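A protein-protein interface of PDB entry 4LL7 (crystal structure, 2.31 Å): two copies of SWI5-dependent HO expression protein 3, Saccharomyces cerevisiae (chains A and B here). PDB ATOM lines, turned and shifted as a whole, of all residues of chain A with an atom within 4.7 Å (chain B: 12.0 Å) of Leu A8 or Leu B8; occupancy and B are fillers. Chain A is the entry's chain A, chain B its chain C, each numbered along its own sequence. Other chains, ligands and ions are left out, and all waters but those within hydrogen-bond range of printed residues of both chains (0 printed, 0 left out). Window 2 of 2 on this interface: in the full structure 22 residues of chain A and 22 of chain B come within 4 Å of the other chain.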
ATOM      1  N   VAL A   4     -37.268  29.271   0.758  1.00  0.00           N
ATOM      2  CA  VAL A   4     -36.213  28.324   1.144  1.00  0.00           C
ATOM      3  C   VAL A   4     -34.988  29.095   1.428  1.00  0.00           C
ATOM      4  O   VAL A   4     -34.563  29.105   2.554  1.00  0.00           O
ATOM      5  CB  VAL A   4     -35.863  27.309   0.003  1.00  0.00           C
ATOM      6  CG1 VAL A   4     -36.957  26.276  -0.048  1.00  0.00           C
ATOM      7  CG2 VAL A   4     -35.710  28.033  -1.382  1.00  0.00           C
ATOM      8  N   ILE A   5     -34.552  29.883   0.445  1.00  0.00           N
ATOM      9  CA  ILE A   5     -33.307  30.643   0.529  1.00  0.00           C
ATOM     10  C   ILE A   5     -33.029  31.616   1.669  1.00  0.00           C
ATOM     11  O   ILE A   5     -32.051  31.447   2.411  1.00  0.00           O
ATOM     12  CB  ILE A   5     -33.031  31.351  -0.832  1.00  0.00           C
ATOM     13  CG1 ILE A   5     -33.184  30.334  -1.974  1.00  0.00           C
ATOM     14  CG2 ILE A   5     -31.618  31.936  -0.851  1.00  0.00           C
ATOM     15  CD1 ILE A   5     -33.095  30.955  -3.355  1.00  0.00           C
ATOM     16  N   GLU A   6     -33.880  32.621   1.801  1.00  0.00           N
ATOM     17  CA  GLU A   6     -33.702  33.621   2.827  1.00  0.00           C
ATOM     18  C   GLU A   6     -34.005  33.095   4.229  1.00  0.00           C
ATOM     19  O   GLU A   6     -33.533  33.655   5.221  1.00  0.00           O
ATOM     20  CB  GLU A   6     -34.538  34.845   2.473  1.00  0.00           C
ATOM     21  CG  GLU A   6     -34.186  35.393   1.087  1.00  0.00           C
ATOM     22  CD  GLU A   6     -34.914  36.676   0.749  1.00  0.00           C
ATOM     23  OE1 GLU A   6     -35.984  36.921   1.342  1.00  0.00           O
ATOM     24  OE2 GLU A   6     -34.427  37.432  -0.120  1.00  0.00           O
ATOM     25  N   SER A   7     -34.795  32.029   4.313  1.00  0.00           N
ATOM     26  CA  SER A   7     -35.073  31.407   5.600  1.00  0.00           C
ATOM     27  C   SER A   7     -33.710  30.835   5.964  1.00  0.00           C
ATOM     28  O   SER A   7     -33.245  30.940   7.099  1.00  0.00           O
ATOM     29  CB  SER A   7     -36.075  30.264   5.444  1.00  0.00           C
ATOM     30  OG  SER A   7     -36.185  29.519   6.643  1.00  0.00           O
ATOM     31  N   LEU A   8     -33.081  30.238   4.953  1.00  0.00           N
ATOM     32  CA  LEU A   8     -31.760  29.636   5.062  1.00  0.00           C
ATOM     33  C   LEU A   8     -30.730  30.687   5.477  1.00  0.00           C
ATOM     34  O   LEU A   8     -29.887  30.434   6.339  1.00  0.00           O
ATOM     35  CB  LEU A   8     -31.384  29.002   3.710  1.00  0.00           C
ATOM     36  CG  LEU A   8     -29.978  28.479   3.408  1.00  0.00           C
ATOM     37  CD1 LEU A   8     -29.398  27.792   4.622  1.00  0.00           C
ATOM     38  CD2 LEU A   8     -30.047  27.517   2.229  1.00  0.00           C
ATOM     39  N   HIS A   9     -30.812  31.871   4.874  1.00  0.00           N
ATOM     40  CA  HIS A   9     -29.889  32.958   5.186  1.00  0.00           C
ATOM     41  C   HIS A   9     -29.994  33.401   6.641  1.00  0.00           C
ATOM     42  O   HIS A   9     -28.977  33.606   7.305  1.00  0.00           O
ATOM     43  CB  HIS A   9     -30.146  34.158   4.269  1.00  0.00           C
ATOM     44  CG  HIS A   9     -29.752  33.927   2.843  1.00  0.00           C
ATOM     45  ND1 HIS A   9     -28.455  33.663   2.461  1.00  0.00           N
ATOM     46  CD2 HIS A   9     -30.485  33.937   1.704  1.00  0.00           C
ATOM     47  CE1 HIS A   9     -28.404  33.520   1.148  1.00  0.00           C
ATOM     48  NE2 HIS A   9     -29.622  33.681   0.665  1.00  0.00           N
ATOM     49  N   ASP A  10     -31.222  33.548   7.135  1.00  0.00           N
ATOM     50  CA  ASP A  10     -31.438  33.964   8.517  1.00  0.00           C
ATOM     51  C   ASP A  10     -30.613  33.128   9.488  1.00  0.00           C
ATOM     52  O   ASP A  10     -30.415  33.515  10.642  1.00  0.00           O
ATOM     53  CB  ASP A  10     -32.919  33.872   8.889  1.00  0.00           C
ATOM     54  CG  ASP A  10     -33.763  34.903   8.167  1.00  0.00           C
ATOM     55  OD1 ASP A  10     -33.197  35.912   7.699  1.00  0.00           O
ATOM     56  OD2 ASP A  10     -34.995  34.712   8.080  1.00  0.00           O
ATOM     57  N   GLN A  11     -30.138  31.980   9.018  1.00  0.00           N
ATOM     58  CA  GLN A  11     -29.314  31.106   9.839  1.00  0.00           C
ATOM     59  C   GLN A  11     -27.840  31.455   9.683  1.00  0.00           C
ATOM     60  O   GLN A  11     -27.086  31.453  10.656  1.00  0.00           O
ATOM     61  CB  GLN A  11     -29.523  29.648   9.454  1.00  0.00           C
ATOM     62  CG  GLN A  11     -30.795  29.041   9.990  1.00  0.00           C
ATOM     63  CD  GLN A  11     -30.604  27.583  10.324  1.00  0.00           C
ATOM     64  OE1 GLN A  11     -30.053  26.826   9.526  1.00  0.00           O
ATOM     65  NE2 GLN A  11     -31.053  27.177  11.508  1.00  0.00           N
ATOM     66  N   ILE A  12     -27.431  31.743   8.451  1.00  0.00           N
ATOM     67  CA  ILE A  12     -26.048  32.104   8.175  1.00  0.00           C
ATOM     68  C   ILE A  12     -25.676  33.359   8.959  1.00  0.00           C
ATOM     69  O   ILE A  12     -24.612  33.418   9.574  1.00  0.00           O
ATOM     70  CB  ILE A  12     -25.827  32.379   6.667  1.00  0.00           C
ATOM     71  CG1 ILE A  12     -26.009  31.091   5.855  1.00  0.00           C
ATOM     72  CG2 ILE A  12     -24.439  32.970   6.447  1.00  0.00           C
ATOM     73  CD1 ILE A  12     -24.805  30.157   5.854  1.00  0.00           C
ATOM     74  N   ILE B   5     -29.300  24.658  -2.755  1.00  0.00           N
ATOM     75  CA  ILE B   5     -29.334  24.777  -1.269  1.00  0.00           C
ATOM     76  C   ILE B   5     -28.217  23.953  -0.638  1.00  0.00           C
ATOM     77  O   ILE B   5     -27.849  24.173   0.515  1.00  0.00           O
ATOM     78  CB  ILE B   5     -30.692  24.298  -0.705  1.00  0.00           C
ATOM     79  CG1 ILE B   5     -31.816  25.188  -1.241  1.00  0.00           C
ATOM     80  CG2 ILE B   5     -30.673  24.334   0.818  1.00  0.00           C
ATOM     81  CD1 ILE B   5     -33.190  24.822  -0.721  1.00  0.00           C
ATOM     82  N   GLU B   6     -27.680  23.006  -1.401  1.00  0.00           N
ATOM     83  CA  GLU B   6     -26.602  22.150  -0.916  1.00  0.00           C
ATOM     84  C   GLU B   6     -25.363  22.978  -0.591  1.00  0.00           C
ATOM     85  O   GLU B   6     -24.690  22.742   0.414  1.00  0.00           O
ATOM     86  CB  GLU B   6     -26.252  21.099  -1.969  1.00  0.00           C
ATOM     87  CG  GLU B   6     -27.423  20.223  -2.380  1.00  0.00           C
ATOM     88  CD  GLU B   6     -27.030  19.170  -3.396  1.00  0.00           C
ATOM     89  OE1 GLU B   6     -26.638  19.542  -4.521  1.00  0.00           O
ATOM     90  OE2 GLU B   6     -27.111  17.969  -3.063  1.00  0.00           O
ATOM     91  N   SER B   7     -25.063  23.944  -1.453  1.00  0.00           N
ATOM     92  CA  SER B   7     -23.910  24.808  -1.252  1.00  0.00           C
ATOM     93  C   SER B   7     -24.098  25.593   0.039  1.00  0.00           C
ATOM     94  O   SER B   7     -23.165  25.748   0.827  1.00  0.00           O
ATOM     95  CB  SER B   7     -23.759  25.774  -2.430  1.00  0.00           C
ATOM     96  OG  SER B   7     -22.616  26.598  -2.278  1.00  0.00           O
ATOM     97  N   LEU B   8     -25.315  26.079   0.255  1.00  0.00           N
ATOM     98  CA  LEU B   8     -25.613  26.848   1.454  1.00  0.00           C
ATOM     99  C   LEU B   8     -25.540  26.003   2.722  1.00  0.00           C
ATOM    100  O   LEU B   8     -25.161  26.503   3.782  1.00  0.00           O
ATOM    101  CB  LEU B   8     -26.988  27.505   1.329  1.00  0.00           C
ATOM    102  CG  LEU B   8     -27.090  28.542   0.206  1.00  0.00           C
ATOM    103  CD1 LEU B   8     -28.426  29.254   0.285  1.00  0.00           C
ATOM    104  CD2 LEU B   8     -25.956  29.551   0.331  1.00  0.00           C
ATOM    105  N   HIS B   9     -25.898  24.726   2.619  1.00  0.00           N
ATOM    106  CA  HIS B   9     -25.839  23.846   3.779  1.00  0.00           C
ATOM    107  C   HIS B   9     -24.369  23.589   4.089  1.00  0.00           C
ATOM    108  O   HIS B   9     -23.975  23.502   5.252  1.00  0.00           O
ATOM    109  CB  HIS B   9     -26.581  22.522   3.506  1.00  0.00           C
ATOM    110  CG  HIS B   9     -25.685  21.361   3.195  1.00  0.00           C
ATOM    111  ND1 HIS B   9     -24.709  20.918   4.064  1.00  0.00           N
ATOM    112  CD2 HIS B   9     -25.633  20.534   2.124  1.00  0.00           C
ATOM    113  CE1 HIS B   9     -24.097  19.871   3.540  1.00  0.00           C
ATOM    114  NE2 HIS B   9     -24.638  19.617   2.363  1.00  0.00           N
ATOM    115  N   ASP B  10     -23.561  23.478   3.039  1.00  0.00           N
ATOM    116  CA  ASP B  10     -22.133  23.237   3.200  1.00  0.00           C
ATOM    117  C   ASP B  10     -21.495  24.420   3.922  1.00  0.00           C
ATOM    118  O   ASP B  10     -20.625  24.245   4.777  1.00  0.00           O
ATOM    119  CB  ASP B  10     -21.471  23.041   1.834  1.00  0.00           C
ATOM    120  CG  ASP B  10     -20.005  22.670   1.946  1.00  0.00           C
ATOM    121  OD1 ASP B  10     -19.493  22.600   3.082  1.00  0.00           O
ATOM    122  OD2 ASP B  10     -19.364  22.449   0.897  1.00  0.00           O
ATOM    123  N   GLN B  11     -21.936  25.625   3.572  1.00  0.00           N
ATOM    124  CA  GLN B  11     -21.421  26.842   4.188  1.00  0.00           C
ATOM    125  C   GLN B  11     -21.838  26.903   5.651  1.00  0.00           C
ATOM    126  O   GLN B  11     -21.068  27.340   6.506  1.00  0.00           O
ATOM    127  CB  GLN B  11     -21.963  28.063   3.459  1.00  0.00           C
ATOM    128  CG  GLN B  11     -21.603  28.113   1.996  1.00  0.00           C
ATOM    129  CD  GLN B  11     -22.390  29.172   1.277  1.00  0.00           C
ATOM    130  OE1 GLN B  11     -22.439  30.320   1.716  1.00  0.00           O
ATOM    131  NE2 GLN B  11     -23.019  28.797   0.168  1.00  0.00           N
ATOM    132  N   ILE B  12     -23.066  26.479   5.931  1.00  0.00           N
ATOM    133  CA  ILE B  12     -23.565  26.463   7.299  1.00  0.00           C
ATOM    134  C   ILE B  12     -22.656  25.532   8.096  1.00  0.00           C
ATOM    135  O   ILE B  12     -22.286  25.833   9.230  1.00  0.00           O
ATOM    136  CB  ILE B  12     -25.016  25.933   7.374  1.00  0.00           C
ATOM    137  CG1 ILE B  12     -25.984  26.943   6.742  1.00  0.00           C
ATOM    138  CG2 ILE B  12     -25.391  25.645   8.822  1.00  0.00           C
ATOM    139  CD1 ILE B  12     -26.328  28.139   7.621  1.00  0.00           C
ATOM    140  N   ASP B  13     -22.296  24.401   7.493  1.00  0.00           N
ATOM    141  CA  ASP B  13     -21.422  23.435   8.151  1.00  0.00           C
ATOM    142  C   ASP B  13     -20.042  24.024   8.411  1.00  0.00           C
ATOM    143  O   ASP B  13     -19.437  23.766   9.451  1.00  0.00           O
ATOM    144  CB  ASP B  13     -21.285  22.163   7.309  1.00  0.00           C
ATOM    145  CG  ASP B  13     -22.489  21.250   7.437  1.00  0.00           C
ATOM    146  OD1 ASP B  13     -22.877  20.936   8.582  1.00  0.00           O
ATOM    147  OD2 ASP B  13     -23.043  20.840   6.395  1.00  0.00           O
ATOM    148  N   MET B  14     -19.542  24.810   7.463  1.00  0.00           N
ATOM    149  CA  MET B  14     -18.236  25.433   7.624  1.00  0.00           C
ATOM    150  C   MET B  14     -18.288  26.467   8.738  1.00  0.00           C
ATOM    151  O   MET B  14     -17.342  26.607   9.512  1.00  0.00           O
ATOM    152  CB  MET B  14     -17.789  26.092   6.319  1.00  0.00           C
ATOM    153  CG  MET B  14     -17.366  25.094   5.260  1.00  0.00           C
ATOM    154  SD  MET B  14     -16.132  23.938   5.899  1.00  0.00           S
ATOM    155  CE  MET B  14     -14.623  24.688   5.305  1.00  0.00           C
ATOM    156  N   LEU B  15     -19.403  27.183   8.820  1.00  0.00           N
ATOM    157  CA  LEU B  15     -19.576  28.202   9.842  1.00  0.00           C
ATOM    158  C   LEU B  15     -19.667  27.554  11.224  1.00  0.00           C
ATOM    159  O   LEU B  15     -19.079  28.050  12.186  1.00  0.00           O
ATOM    160  CB  LEU B  15     -20.830  29.028   9.544  1.00  0.00           C
ATOM    161  CG  LEU B  15     -20.722  30.541   9.749  1.00  0.00           C
ATOM    162  CD1 LEU B  15     -19.417  31.046   9.157  1.00  0.00           C
ATOM    163  CD2 LEU B  15     -21.904  31.235   9.091  1.00  0.00           C
ATOM    164  N   THR B  16     -20.391  26.441  11.320  1.00  0.00           N
ATOM    165  CA  THR B  16     -20.533  25.738  12.593  1.00  0.00           C
ATOM    166  C   THR B  16     -19.187  25.196  13.058  1.00  0.00           C
ATOM    167  O   THR B  16     -18.917  25.124  14.257  1.00  0.00           O
ATOM    168  CB  THR B  16     -21.526  24.562  12.495  1.00  0.00           C
ATOM    169  OG1 THR B  16     -21.133  23.688  11.429  1.00  0.00           O
ATOM    170  CG2 THR B  16     -22.938  25.074  12.253  1.00  0.00           C
ATOM    171  N   LYS B  17     -18.347  24.805  12.106  1.00  0.00           N
ATOM    172  CA  LYS B  17     -17.028  24.295  12.444  1.00  0.00           C
ATOM    173  C   LYS B  17     -16.171  25.453  12.934  1.00  0.00           C
ATOM    174  O   LYS B  17     -15.371  25.299  13.856  1.00  0.00           O
ATOM    175  CB  LYS B  17     -16.371  23.635  11.229  1.00  0.00           C
ATOM    176  CG  LYS B  17     -17.008  22.319  10.841  1.00  0.00           C
ATOM    177  CD  LYS B  17     -16.146  21.552   9.857  1.00  0.00           C
ATOM    178  CE  LYS B  17     -16.780  20.209   9.520  1.00  0.00           C
ATOM    179  NZ  LYS B  17     -15.943  19.403   8.590  1.00  0.00           N
ATOM    180  N   THR B  18     -16.350  26.616  12.319  1.00  0.00           N
ATOM    181  CA  THR B  18     -15.591  27.789  12.713  1.00  0.00           C
ATOM    182  C   THR B  18     -15.975  28.188  14.133  1.00  0.00           C
ATOM    183  O   THR B  18     -15.102  28.399  14.972  1.00  0.00           O
ATOM    184  CB  THR B  18     -15.848  28.980  11.767  1.00  0.00           C
ATOM    185  OG1 THR B  18     -15.631  28.570  10.412  1.00  0.00           O
ATOM    186  CG2 THR B  18     -14.895  30.124  12.084  1.00  0.00           C
ATOM    187  N   ASN B  19     -17.275  28.268  14.413  1.00  0.00           N
ATOM    188  CA  ASN B  19     -17.731  28.655  15.745  1.00  0.00           C
ATOM    189  C   ASN B  19     -17.298  27.680  16.839  1.00  0.00           C
ATOM    190  O   ASN B  19     -16.981  28.096  17.954  1.00  0.00           O
ATOM    191  CB  ASN B  19     -19.261  28.822  15.782  1.00  0.00           C
ATOM    192  CG  ASN B  19     -20.008  27.512  15.595  1.00  0.00           C
ATOM    193  OD1 ASN B  19     -19.688  26.497  16.219  1.00  0.00           O
ATOM    194  ND2 ASN B  19     -21.031  27.537  14.747  1.00  0.00           N
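Val A4 touches Ile B5 (CB to CD1, 3.7 Å). Leu A8 touches Ile B5. Leu A8 touches Leu B8 (CD2 to CD1, 3.1 Å). Gln A11 touches Ile B12. Ile A12 touches Ile B12. Ile A12 touches Leu B15 (O to CD2, 3.5 Å).
The backbone carbonyl oxygen (O) of Ile B12 lies close to the side-chain hydroxyl (OG1) of Thr B16. The backbone carbonyl oxygen (O) of Leu B15 is in hydrogen-bond range of the side-chain amide nitrogen (ND2) of Asn B19 (3.3 Å).
Hydrophobic or aromatic side chains of chain A within 4 Å of the printed part of chain B: Val A4, Leu A8 and Ile A12. Of the 15 printed residues of chain B, 4 touch a printed residue of chain A. Printed residues of chain B that touch a printed residue of chain A: Ile B5, Leu B8, Ile B12 and Leu B15.
Leu A8 touches Ile B5, but with the chains exchanged Ile A5 does not touch Leu B8 (4.3 Å). Leu A8 touches its own counterpart, Leu B8. Gln A11 touches Ile B12, but with the chains exchanged Ile A12 does not touch Gln B11 (4.3 Å). Ile B12 touches its own counterpart, Ile A12. Of the 6 pairs that touch across the chains among the printed residues, 2 have their exchanged pair printed and touching as well.
Leu A8 touches just these residues of chain B: Ile B5 (3.5 Å) and Leu B8 (3.1 Å). Of chain A, only Leu A8 (3.1 Å) comes within 4 Å of Leu B8. Of chain B, only Ile B5 comes within 4 Å of Val A4. No residue of chain B comes within 4 Å of Ile A5. No residue of chain B comes within 4 Å of Ser A7. No residue of chain B comes within 4 Å of Asp A10. Printed residues of chain A within 4 Å of Ile B5: Val A4 and Leu A8. Of the printed residues of chain B, Gln A11 touches Ile B12 (3.98 Å). Printed residues of chain A within 4 Å of Leu B15: Ile A12 (3.5 Å). Printed residues of chain A within 4 Å of Ile B12: Gln A11 and Ile A12. The nearest residue of chain A that does not touch Leu B8 is Ile A12 (4.2 Å). The nearest printed residue of chain A that does not touch Ile B5 is Ile A5 (5.4 Å).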
